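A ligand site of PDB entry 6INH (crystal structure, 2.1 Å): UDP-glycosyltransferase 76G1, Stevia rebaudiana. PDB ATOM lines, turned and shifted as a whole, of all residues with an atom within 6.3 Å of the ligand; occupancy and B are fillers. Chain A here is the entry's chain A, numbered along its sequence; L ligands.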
ATOM      1  N   LYS A 223      15.196  23.298   6.092  1.00  0.00           N
ATOM      2  CA  LYS A 223      15.942  23.122   4.846  1.00  0.00           C
ATOM      3  C   LYS A 223      15.037  22.835   3.661  1.00  0.00           C
ATOM      4  O   LYS A 223      15.215  23.426   2.599  1.00  0.00           O
ATOM      5  CB  LYS A 223      16.967  22.002   5.017  1.00  0.00           C
ATOM      6  CG  LYS A 223      17.857  21.703   3.818  1.00  0.00           C
ATOM      7  CD  LYS A 223      18.793  20.536   4.153  1.00  0.00           C
ATOM      8  CE  LYS A 223      19.874  20.309   3.110  1.00  0.00           C
ATOM      9  NZ  LYS A 223      19.330  19.589   1.931  1.00  0.00           N
ATOM     10  N   GLU A 224      14.037  21.984   3.874  1.00  0.00           N
ATOM     11  CA  GLU A 224      13.189  21.502   2.805  1.00  0.00           C
ATOM     12  C   GLU A 224      12.154  22.562   2.434  1.00  0.00           C
ATOM     13  O   GLU A 224      11.418  22.401   1.486  1.00  0.00           O
ATOM     14  CB  GLU A 224      12.525  20.162   3.194  1.00  0.00           C
ATOM     15  CG  GLU A 224      13.514  18.992   3.413  1.00  0.00           C
ATOM     16  CD  GLU A 224      14.346  19.074   4.705  1.00  0.00           C
ATOM     17  OE1 GLU A 224      14.028  19.864   5.658  1.00  0.00           O
ATOM     18  OE2 GLU A 224      15.362  18.341   4.781  1.00  0.00           O
ATOM     19  N   LEU A 230      19.797  27.984   0.258  1.00  0.00           N
ATOM     20  CA  LEU A 230      20.807  27.550   1.207  1.00  0.00           C
ATOM     21  C   LEU A 230      22.236  27.863   0.771  1.00  0.00           C
ATOM     22  O   LEU A 230      23.056  28.287   1.599  1.00  0.00           O
ATOM     23  CB  LEU A 230      20.657  26.048   1.464  1.00  0.00           C
ATOM     24  CG  LEU A 230      21.282  25.415   2.695  1.00  0.00           C
ATOM     25  CD1 LEU A 230      20.888  26.150   3.960  1.00  0.00           C
ATOM     26  CD2 LEU A 230      20.853  23.952   2.751  1.00  0.00           C
ATOM     27  N   ILE A 234      25.197  29.978   2.881  1.00  0.00           N
ATOM     28  CA  ILE A 234      26.499  29.374   3.140  1.00  0.00           C
ATOM     29  C   ILE A 234      27.617  30.209   2.517  1.00  0.00           C
ATOM     30  O   ILE A 234      28.672  30.380   3.123  1.00  0.00           O
ATOM     31  CB  ILE A 234      26.555  27.906   2.655  1.00  0.00           C
ATOM     32  CG1 ILE A 234      25.604  27.042   3.489  1.00  0.00           C
ATOM     33  CG2 ILE A 234      27.980  27.340   2.741  1.00  0.00           C
ATOM     34  CD1 ILE A 234      25.288  25.694   2.871  1.00  0.00           C
ATOM     35  N   PRO A 240      28.495  29.507  11.173  1.00  0.00           N
ATOM     36  CA  PRO A 240      27.498  28.485  10.878  1.00  0.00           C
ATOM     37  C   PRO A 240      26.044  28.998  10.923  1.00  0.00           C
ATOM     38  O   PRO A 240      25.715  29.897  11.717  1.00  0.00           O
ATOM     39  CB  PRO A 240      27.734  27.418  11.961  1.00  0.00           C
ATOM     40  CG  PRO A 240      28.579  28.052  12.998  1.00  0.00           C
ATOM     41  CD  PRO A 240      29.302  29.192  12.354  1.00  0.00           C
ATOM     42  N   SER A 241      25.221  28.419  10.068  1.00  0.00           N
ATOM     43  CA  SER A 241      23.785  28.669  10.020  1.00  0.00           C
ATOM     44  C   SER A 241      23.054  27.436  10.517  1.00  0.00           C
ATOM     45  O   SER A 241      23.460  26.289  10.252  1.00  0.00           O
ATOM     46  CB  SER A 241      23.320  28.999   8.588  1.00  0.00           C
ATOM     47  OG  SER A 241      23.585  30.343   8.258  1.00  0.00           O
ATOM     48  N   PHE A 242      21.974  27.659  11.260  1.00  0.00           N
ATOM     49  CA  PHE A 242      21.220  26.597  11.883  1.00  0.00           C
ATOM     50  C   PHE A 242      19.769  26.847  11.513  1.00  0.00           C
ATOM     51  O   PHE A 242      19.252  27.934  11.788  1.00  0.00           O
ATOM     52  CB  PHE A 242      21.397  26.612  13.405  1.00  0.00           C
ATOM     53  CG  PHE A 242      22.812  26.655  13.869  1.00  0.00           C
ATOM     54  CD1 PHE A 242      23.469  27.892  14.040  1.00  0.00           C
ATOM     55  CD2 PHE A 242      23.511  25.482  14.114  1.00  0.00           C
ATOM     56  CE1 PHE A 242      24.787  27.924  14.465  1.00  0.00           C
ATOM     57  CE2 PHE A 242      24.831  25.530  14.541  1.00  0.00           C
ATOM     58  CZ  PHE A 242      25.460  26.756  14.728  1.00  0.00           C
ATOM     59  N   LEU A 243      19.109  25.878  10.890  1.00  0.00           N
ATOM     60  CA  LEU A 243      17.720  26.059  10.407  1.00  0.00           C
ATOM     61  C   LEU A 243      16.811  25.279  11.310  1.00  0.00           C
ATOM     62  O   LEU A 243      16.776  24.057  11.212  1.00  0.00           O
ATOM     63  CB  LEU A 243      17.535  25.581   8.948  1.00  0.00           C
ATOM     64  CG  LEU A 243      17.921  26.593   7.867  1.00  0.00           C
ATOM     65  CD1 LEU A 243      19.405  26.930   7.932  1.00  0.00           C
ATOM     66  CD2 LEU A 243      17.566  26.051   6.484  1.00  0.00           C
ATOM     67  N   GLY A 441      18.448  12.483  12.335  1.00  0.00           N
ATOM     68  CA  GLY A 441      18.955  12.541  10.969  1.00  0.00           C
ATOM     69  C   GLY A 441      18.350  13.639  10.115  1.00  0.00           C
ATOM     70  O   GLY A 441      18.863  13.924   9.045  1.00  0.00           O
ATOM     71  N   GLY A 442      17.260  14.267  10.584  1.00  0.00           N
ATOM     72  CA  GLY A 442      16.642  15.341   9.847  1.00  0.00           C
ATOM     73  C   GLY A 442      17.417  16.640   9.924  1.00  0.00           C
ATOM     74  O   GLY A 442      18.218  16.842  10.828  1.00  0.00           O
ATOM     75  N   SER A 443      17.166  17.508   8.954  1.00  0.00           N
ATOM     76  CA  SER A 443      17.885  18.780   8.835  1.00  0.00           C
ATOM     77  C   SER A 443      17.701  19.655  10.083  1.00  0.00           C
ATOM     78  O   SER A 443      18.649  20.299  10.524  1.00  0.00           O
ATOM     79  CB  SER A 443      17.384  19.536   7.598  1.00  0.00           C
ATOM     80  OG  SER A 443      15.998  19.853   7.717  1.00  0.00           O
ATOM     81  N   SER A 444      16.490  19.658  10.636  1.00  0.00           N
ATOM     82  CA  SER A 444      16.162  20.508  11.804  1.00  0.00           C
ATOM     83  C   SER A 444      16.718  19.928  13.087  1.00  0.00           C
ATOM     84  O   SER A 444      17.264  20.671  13.937  1.00  0.00           O
ATOM     85  CB  SER A 444      14.635  20.701  11.912  1.00  0.00           C
ATOM     86  OG  SER A 444      14.128  21.311  10.742  1.00  0.00           O
ATOM     87  N   GLU A 446      19.362  17.989  13.218  1.00  0.00           N
ATOM     88  CA  GLU A 446      20.815  18.170  13.172  1.00  0.00           C
ATOM     89  C   GLU A 446      21.223  19.631  13.437  1.00  0.00           C
ATOM     90  O   GLU A 446      22.214  19.883  14.124  1.00  0.00           O
ATOM     91  CB  GLU A 446      21.373  17.657  11.846  1.00  0.00           C
ATOM     92  CG  GLU A 446      21.179  16.155  11.623  1.00  0.00           C
ATOM     93  CD  GLU A 446      21.855  15.241  12.674  1.00  0.00           C
ATOM     94  OE1 GLU A 446      22.787  15.694  13.362  1.00  0.00           O
ATOM     95  OE2 GLU A 446      21.437  14.059  12.798  1.00  0.00           O
ATOM     96  N   SER A 447      20.430  20.579  12.942  1.00  0.00           N
ATOM     97  CA  SER A 447      20.622  22.000  13.225  1.00  0.00           C
ATOM     98  C   SER A 447      20.584  22.293  14.699  1.00  0.00           C
ATOM     99  O   SER A 447      21.467  23.009  15.211  1.00  0.00           O
ATOM    100  CB  SER A 447      19.568  22.854  12.538  1.00  0.00           C
ATOM    101  OG  SER A 447      19.888  23.022  11.196  1.00  0.00           O
ATOM    102  N   LEU A 448      19.577  21.754  15.376  1.00  0.00           N
ATOM    103  CA  LEU A 448      19.418  21.993  16.825  1.00  0.00           C
ATOM    104  C   LEU A 448      20.506  21.304  17.634  1.00  0.00           C
ATOM    105  O   LEU A 448      21.056  21.927  18.575  1.00  0.00           O
ATOM    106  CB  LEU A 448      18.038  21.600  17.324  1.00  0.00           C
ATOM    107  CG  LEU A 448      17.768  21.831  18.821  1.00  0.00           C
ATOM    108  CD1 LEU A 448      18.025  23.277  19.240  1.00  0.00           C
ATOM    109  CD2 LEU A 448      16.365  21.411  19.179  1.00  0.00           C
ATOM    110  N   GLU A 449      20.837  20.048  17.289  1.00  0.00           N
ATOM    111  CA  GLU A 449      21.935  19.366  17.978  1.00  0.00           C
ATOM    112  C   GLU A 449      23.264  20.104  17.808  1.00  0.00           C
ATOM    113  O   GLU A 449      24.012  20.233  18.766  1.00  0.00           O
ATOM    114  CB  GLU A 449      22.103  17.895  17.546  1.00  0.00           C
ATOM    115  CG  GLU A 449      20.920  17.004  17.903  1.00  0.00           C
ATOM    116  CD  GLU A 449      20.492  17.106  19.357  1.00  0.00           C
ATOM    117  OE1 GLU A 449      21.308  16.799  20.235  1.00  0.00           O
ATOM    118  OE2 GLU A 449      19.326  17.499  19.621  1.00  0.00           O
ATOM    119  N   SER A 450      23.530  20.569  16.592  1.00  0.00           N
ATOM    120  CA  SER A 450      24.754  21.298  16.300  1.00  0.00           C
ATOM    121  C   SER A 450      24.785  22.665  16.981  1.00  0.00           C
ATOM    122  O   SER A 450      25.847  23.101  17.399  1.00  0.00           O
ATOM    123  CB  SER A 450      24.911  21.485  14.796  1.00  0.00           C
ATOM    124  OG  SER A 450      25.075  20.227  14.182  1.00  0.00           O
ATOM    125  N   LEU A 451      23.648  23.341  17.046  1.00  0.00           N
ATOM    126  CA  LEU A 451      23.558  24.620  17.738  1.00  0.00           C
ATOM    127  C   LEU A 451      23.916  24.481  19.220  1.00  0.00           C
ATOM    128  O   LEU A 451      24.668  25.295  19.759  1.00  0.00           O
ATOM    129  CB  LEU A 451      22.163  25.257  17.596  1.00  0.00           C
ATOM    130  CG  LEU A 451      21.940  26.588  18.340  1.00  0.00           C
ATOM    131  CD1 LEU A 451      22.843  27.674  17.768  1.00  0.00           C
ATOM    132  CD2 LEU A 451      20.480  27.018  18.246  1.00  0.00           C
ATOM    133  N   SER A 453      25.704  22.040  20.713  1.00  0.00           N
ATOM    134  CA  SER A 453      27.131  21.706  20.817  1.00  0.00           C
ATOM    135  C   SER A 453      28.022  22.922  20.530  1.00  0.00           C
ATOM    136  O   SER A 453      29.020  23.148  21.233  1.00  0.00           O
ATOM    137  CB  SER A 453      27.502  20.577  19.852  1.00  0.00           C
ATOM    138  OG  SER A 453      26.699  19.443  20.080  1.00  0.00           O
ATOM    139  N   TYR A 454      27.663  23.686  19.513  1.00  0.00           N
ATOM    140  CA  TYR A 454      28.377  24.903  19.157  1.00  0.00           C
ATOM    141  C   TYR A 454      28.339  25.935  20.280  1.00  0.00           C
ATOM    142  O   TYR A 454      29.383  26.430  20.671  1.00  0.00           O
ATOM    143  CB  TYR A 454      27.807  25.485  17.875  1.00  0.00           C
ATOM    144  CG  TYR A 454      28.536  26.701  17.376  1.00  0.00           C
ATOM    145  CD1 TYR A 454      29.855  26.611  16.920  1.00  0.00           C
ATOM    146  CD2 TYR A 454      27.906  27.949  17.347  1.00  0.00           C
ATOM    147  CE1 TYR A 454      30.530  27.742  16.465  1.00  0.00           C
ATOM    148  CE2 TYR A 454      28.551  29.066  16.892  1.00  0.00           C
ATOM    149  CZ  TYR A 454      29.877  28.957  16.444  1.00  0.00           C
ATOM    150  OH  TYR A 454      30.522  30.088  15.975  1.00  0.00           O
ATOM    151  N   ILE A 455      27.160  26.227  20.810  1.00  0.00           N
ATOM    152  CA  ILE A 455      27.041  27.171  21.915  1.00  0.00           C
ATOM    153  C   ILE A 455      27.869  26.694  23.104  1.00  0.00           C
ATOM    154  O   ILE A 455      28.621  27.487  23.665  1.00  0.00           O
ATOM    155  CB  ILE A 455      25.595  27.463  22.333  1.00  0.00           C
ATOM    156  CG1 ILE A 455      24.891  28.257  21.247  1.00  0.00           C
ATOM    157  CG2 ILE A 455      25.546  28.274  23.630  1.00  0.00           C
ATOM    158  CD1 ILE A 455      23.383  28.306  21.395  1.00  0.00           C
ATOM    159  N   SER A 457      30.479  24.971  23.196  1.00  0.00           N
ATOM    160  CA  SER A 457      31.917  25.063  22.920  1.00  0.00           C
ATOM    161  C   SER A 457      32.467  26.488  22.910  1.00  0.00           C
ATOM    162  O   SER A 457      33.697  26.641  22.864  1.00  0.00           O
ATOM    163  CB  SER A 457      32.205  24.452  21.538  1.00  0.00           C
ATOM    164  OG  SER A 457      31.795  25.363  20.513  1.00  0.00           O
HETATM  165  C1  LIG L   1      27.918  23.744  12.584  1.00  0.00           C
HETATM  166  C2  LIG L   1      27.303  22.039  10.851  1.00  0.00           C
HETATM  167  C3  LIG L   1      25.571  23.540  11.763  1.00  0.00           C
HETATM  168  C4  LIG L   1      22.131  18.580   7.211  1.00  0.00           C
HETATM  169  C5  LIG L   1      22.741  16.247   7.882  1.00  0.00           C
HETATM  170  C6  LIG L   1      20.840  16.746   6.322  1.00  0.00           C
HETATM  171  C7  LIG L   1      21.931  21.003   6.882  1.00  0.00           C
HETATM  172  C8  LIG L   1      20.322  22.377   8.020  1.00  0.00           C
HETATM  173  C9  LIG L   1      23.563  22.343  10.971  1.00  0.00           C
HETATM  174  C10 LIG L   1      19.417  16.434   5.886  1.00  0.00           C
HETATM  175  C11 LIG L   1      25.009  22.660  10.637  1.00  0.00           C
HETATM  176  C12 LIG L   1      25.924  21.430  10.656  1.00  0.00           C
HETATM  177  C13 LIG L   1      27.715  22.648   9.524  1.00  0.00           C
HETATM  178  C14 LIG L   1      28.148  20.405  12.525  1.00  0.00           C
HETATM  179  O1  LIG L   1      19.108  17.194   4.711  1.00  0.00           O
HETATM  180  C15 LIG L   1      21.341  15.817   7.429  1.00  0.00           C
HETATM  181  O2  LIG L   1      21.402  14.464   6.959  1.00  0.00           O
HETATM  182  O3  LIG L   1      23.205  15.465   8.979  1.00  0.00           O
HETATM  183  O4  LIG L   1      20.863  18.106   6.769  1.00  0.00           O
HETATM  184  O5  LIG L   1      21.924  19.868   7.784  1.00  0.00           O
HETATM  185  C16 LIG L   1      22.708  17.704   8.313  1.00  0.00           C
HETATM  186  O6  LIG L   1      24.021  18.142   8.662  1.00  0.00           O
HETATM  187  O7  LIG L   1      28.641  22.424  16.190  1.00  0.00           O
HETATM  188  C17 LIG L   1      29.390  21.237  15.913  1.00  0.00           C
HETATM  189  C18 LIG L   1      28.661  20.418  14.848  1.00  0.00           C
HETATM  190  C19 LIG L   1      29.041  18.945  14.865  1.00  0.00           C
HETATM  191  O8  LIG L   1      28.556  18.351  16.080  1.00  0.00           O
HETATM  192  C20 LIG L   1      28.469  18.178  13.668  1.00  0.00           C
HETATM  193  O9  LIG L   1      29.154  16.928  13.526  1.00  0.00           O
HETATM  194  O10 LIG L   1      28.957  20.974  13.554  1.00  0.00           O
HETATM  195  C21 LIG L   1      28.561  18.949  12.348  1.00  0.00           C
HETATM  196  O11 LIG L   1      27.709  18.341  11.365  1.00  0.00           O
HETATM  197  O12 LIG L   1      22.033  20.836   5.674  1.00  0.00           O
HETATM  198  C22 LIG L   1      21.772  22.376   7.511  1.00  0.00           C
HETATM  199  C23 LIG L   1      21.823  23.492   6.478  1.00  0.00           C
HETATM  200  C24 LIG L   1      22.846  22.653   8.603  1.00  0.00           C
HETATM  201  C25 LIG L   1      22.847  21.685   9.812  1.00  0.00           C
HETATM  202  C26 LIG L   1      27.030  23.152  11.814  1.00  0.00           C
HETATM  203  C27 LIG L   1      26.684  23.652   8.944  1.00  0.00           C
HETATM  204  C28 LIG L   1      25.174  23.413   9.271  1.00  0.00           C
HETATM  205  C29 LIG L   1      24.303  22.876   8.090  1.00  0.00           C
HETATM  206  C30 LIG L   1      24.917  21.593   7.437  1.00  0.00           C
HETATM  207  C31 LIG L   1      24.271  23.936   6.987  1.00  0.00           C
HETATM  208  C32 LIG L   1      23.206  23.743   5.909  1.00  0.00           C
HETATM  209  O13 LIG L   1      28.312  21.109  11.279  1.00  0.00           O
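O7 of the ligand sits at hydrogen-bond distance from O of Ser 450 (3.1 Å).
The backbone carbonyl oxygen (O) of Gly 441 is in hydrogen-bond range of an oxygen (O2) of the ligand.
Merely in contact with the ligand: Ser 447, Lys 223, Glu 446, Ser 241, Phe 242, Tyr 454, Ser 443, Pro 240, Leu 230 and Glu 224.
Hydrophobic or aromatic side chains within 4 Å of the ligand: Leu 230, Pro 240, Phe 242 and Tyr 454.
Within 4 Å of the ligand: Lys 223, Glu 224, Leu 230, Pro 240, Ser 241, Phe 242, Gly 441, Ser 443, Glu 446, Ser 447, Ser 450 and Tyr 454.
OG of Ser 457 lies within hydrogen-bond range of O of Tyr 454 (2.6 Å).
OG of Ser 450 lies within hydrogen-bond range of O of Glu 446 (2.9 Å).
OG of Ser 447 lies within hydrogen-bond range of O of Ser 443, at 3.1 Å.
The side-chain carboxylate (OE2) of Glu 446 is in hydrogen-bond range of the backbone NH (N) of Gly 441 (3.4 Å).
OE1 of Glu 224 is in hydrogen-bond range of OG of Ser 443 (2.8 Å).
OG of Ser 447 is in hydrogen-bond range of N of Leu 243.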
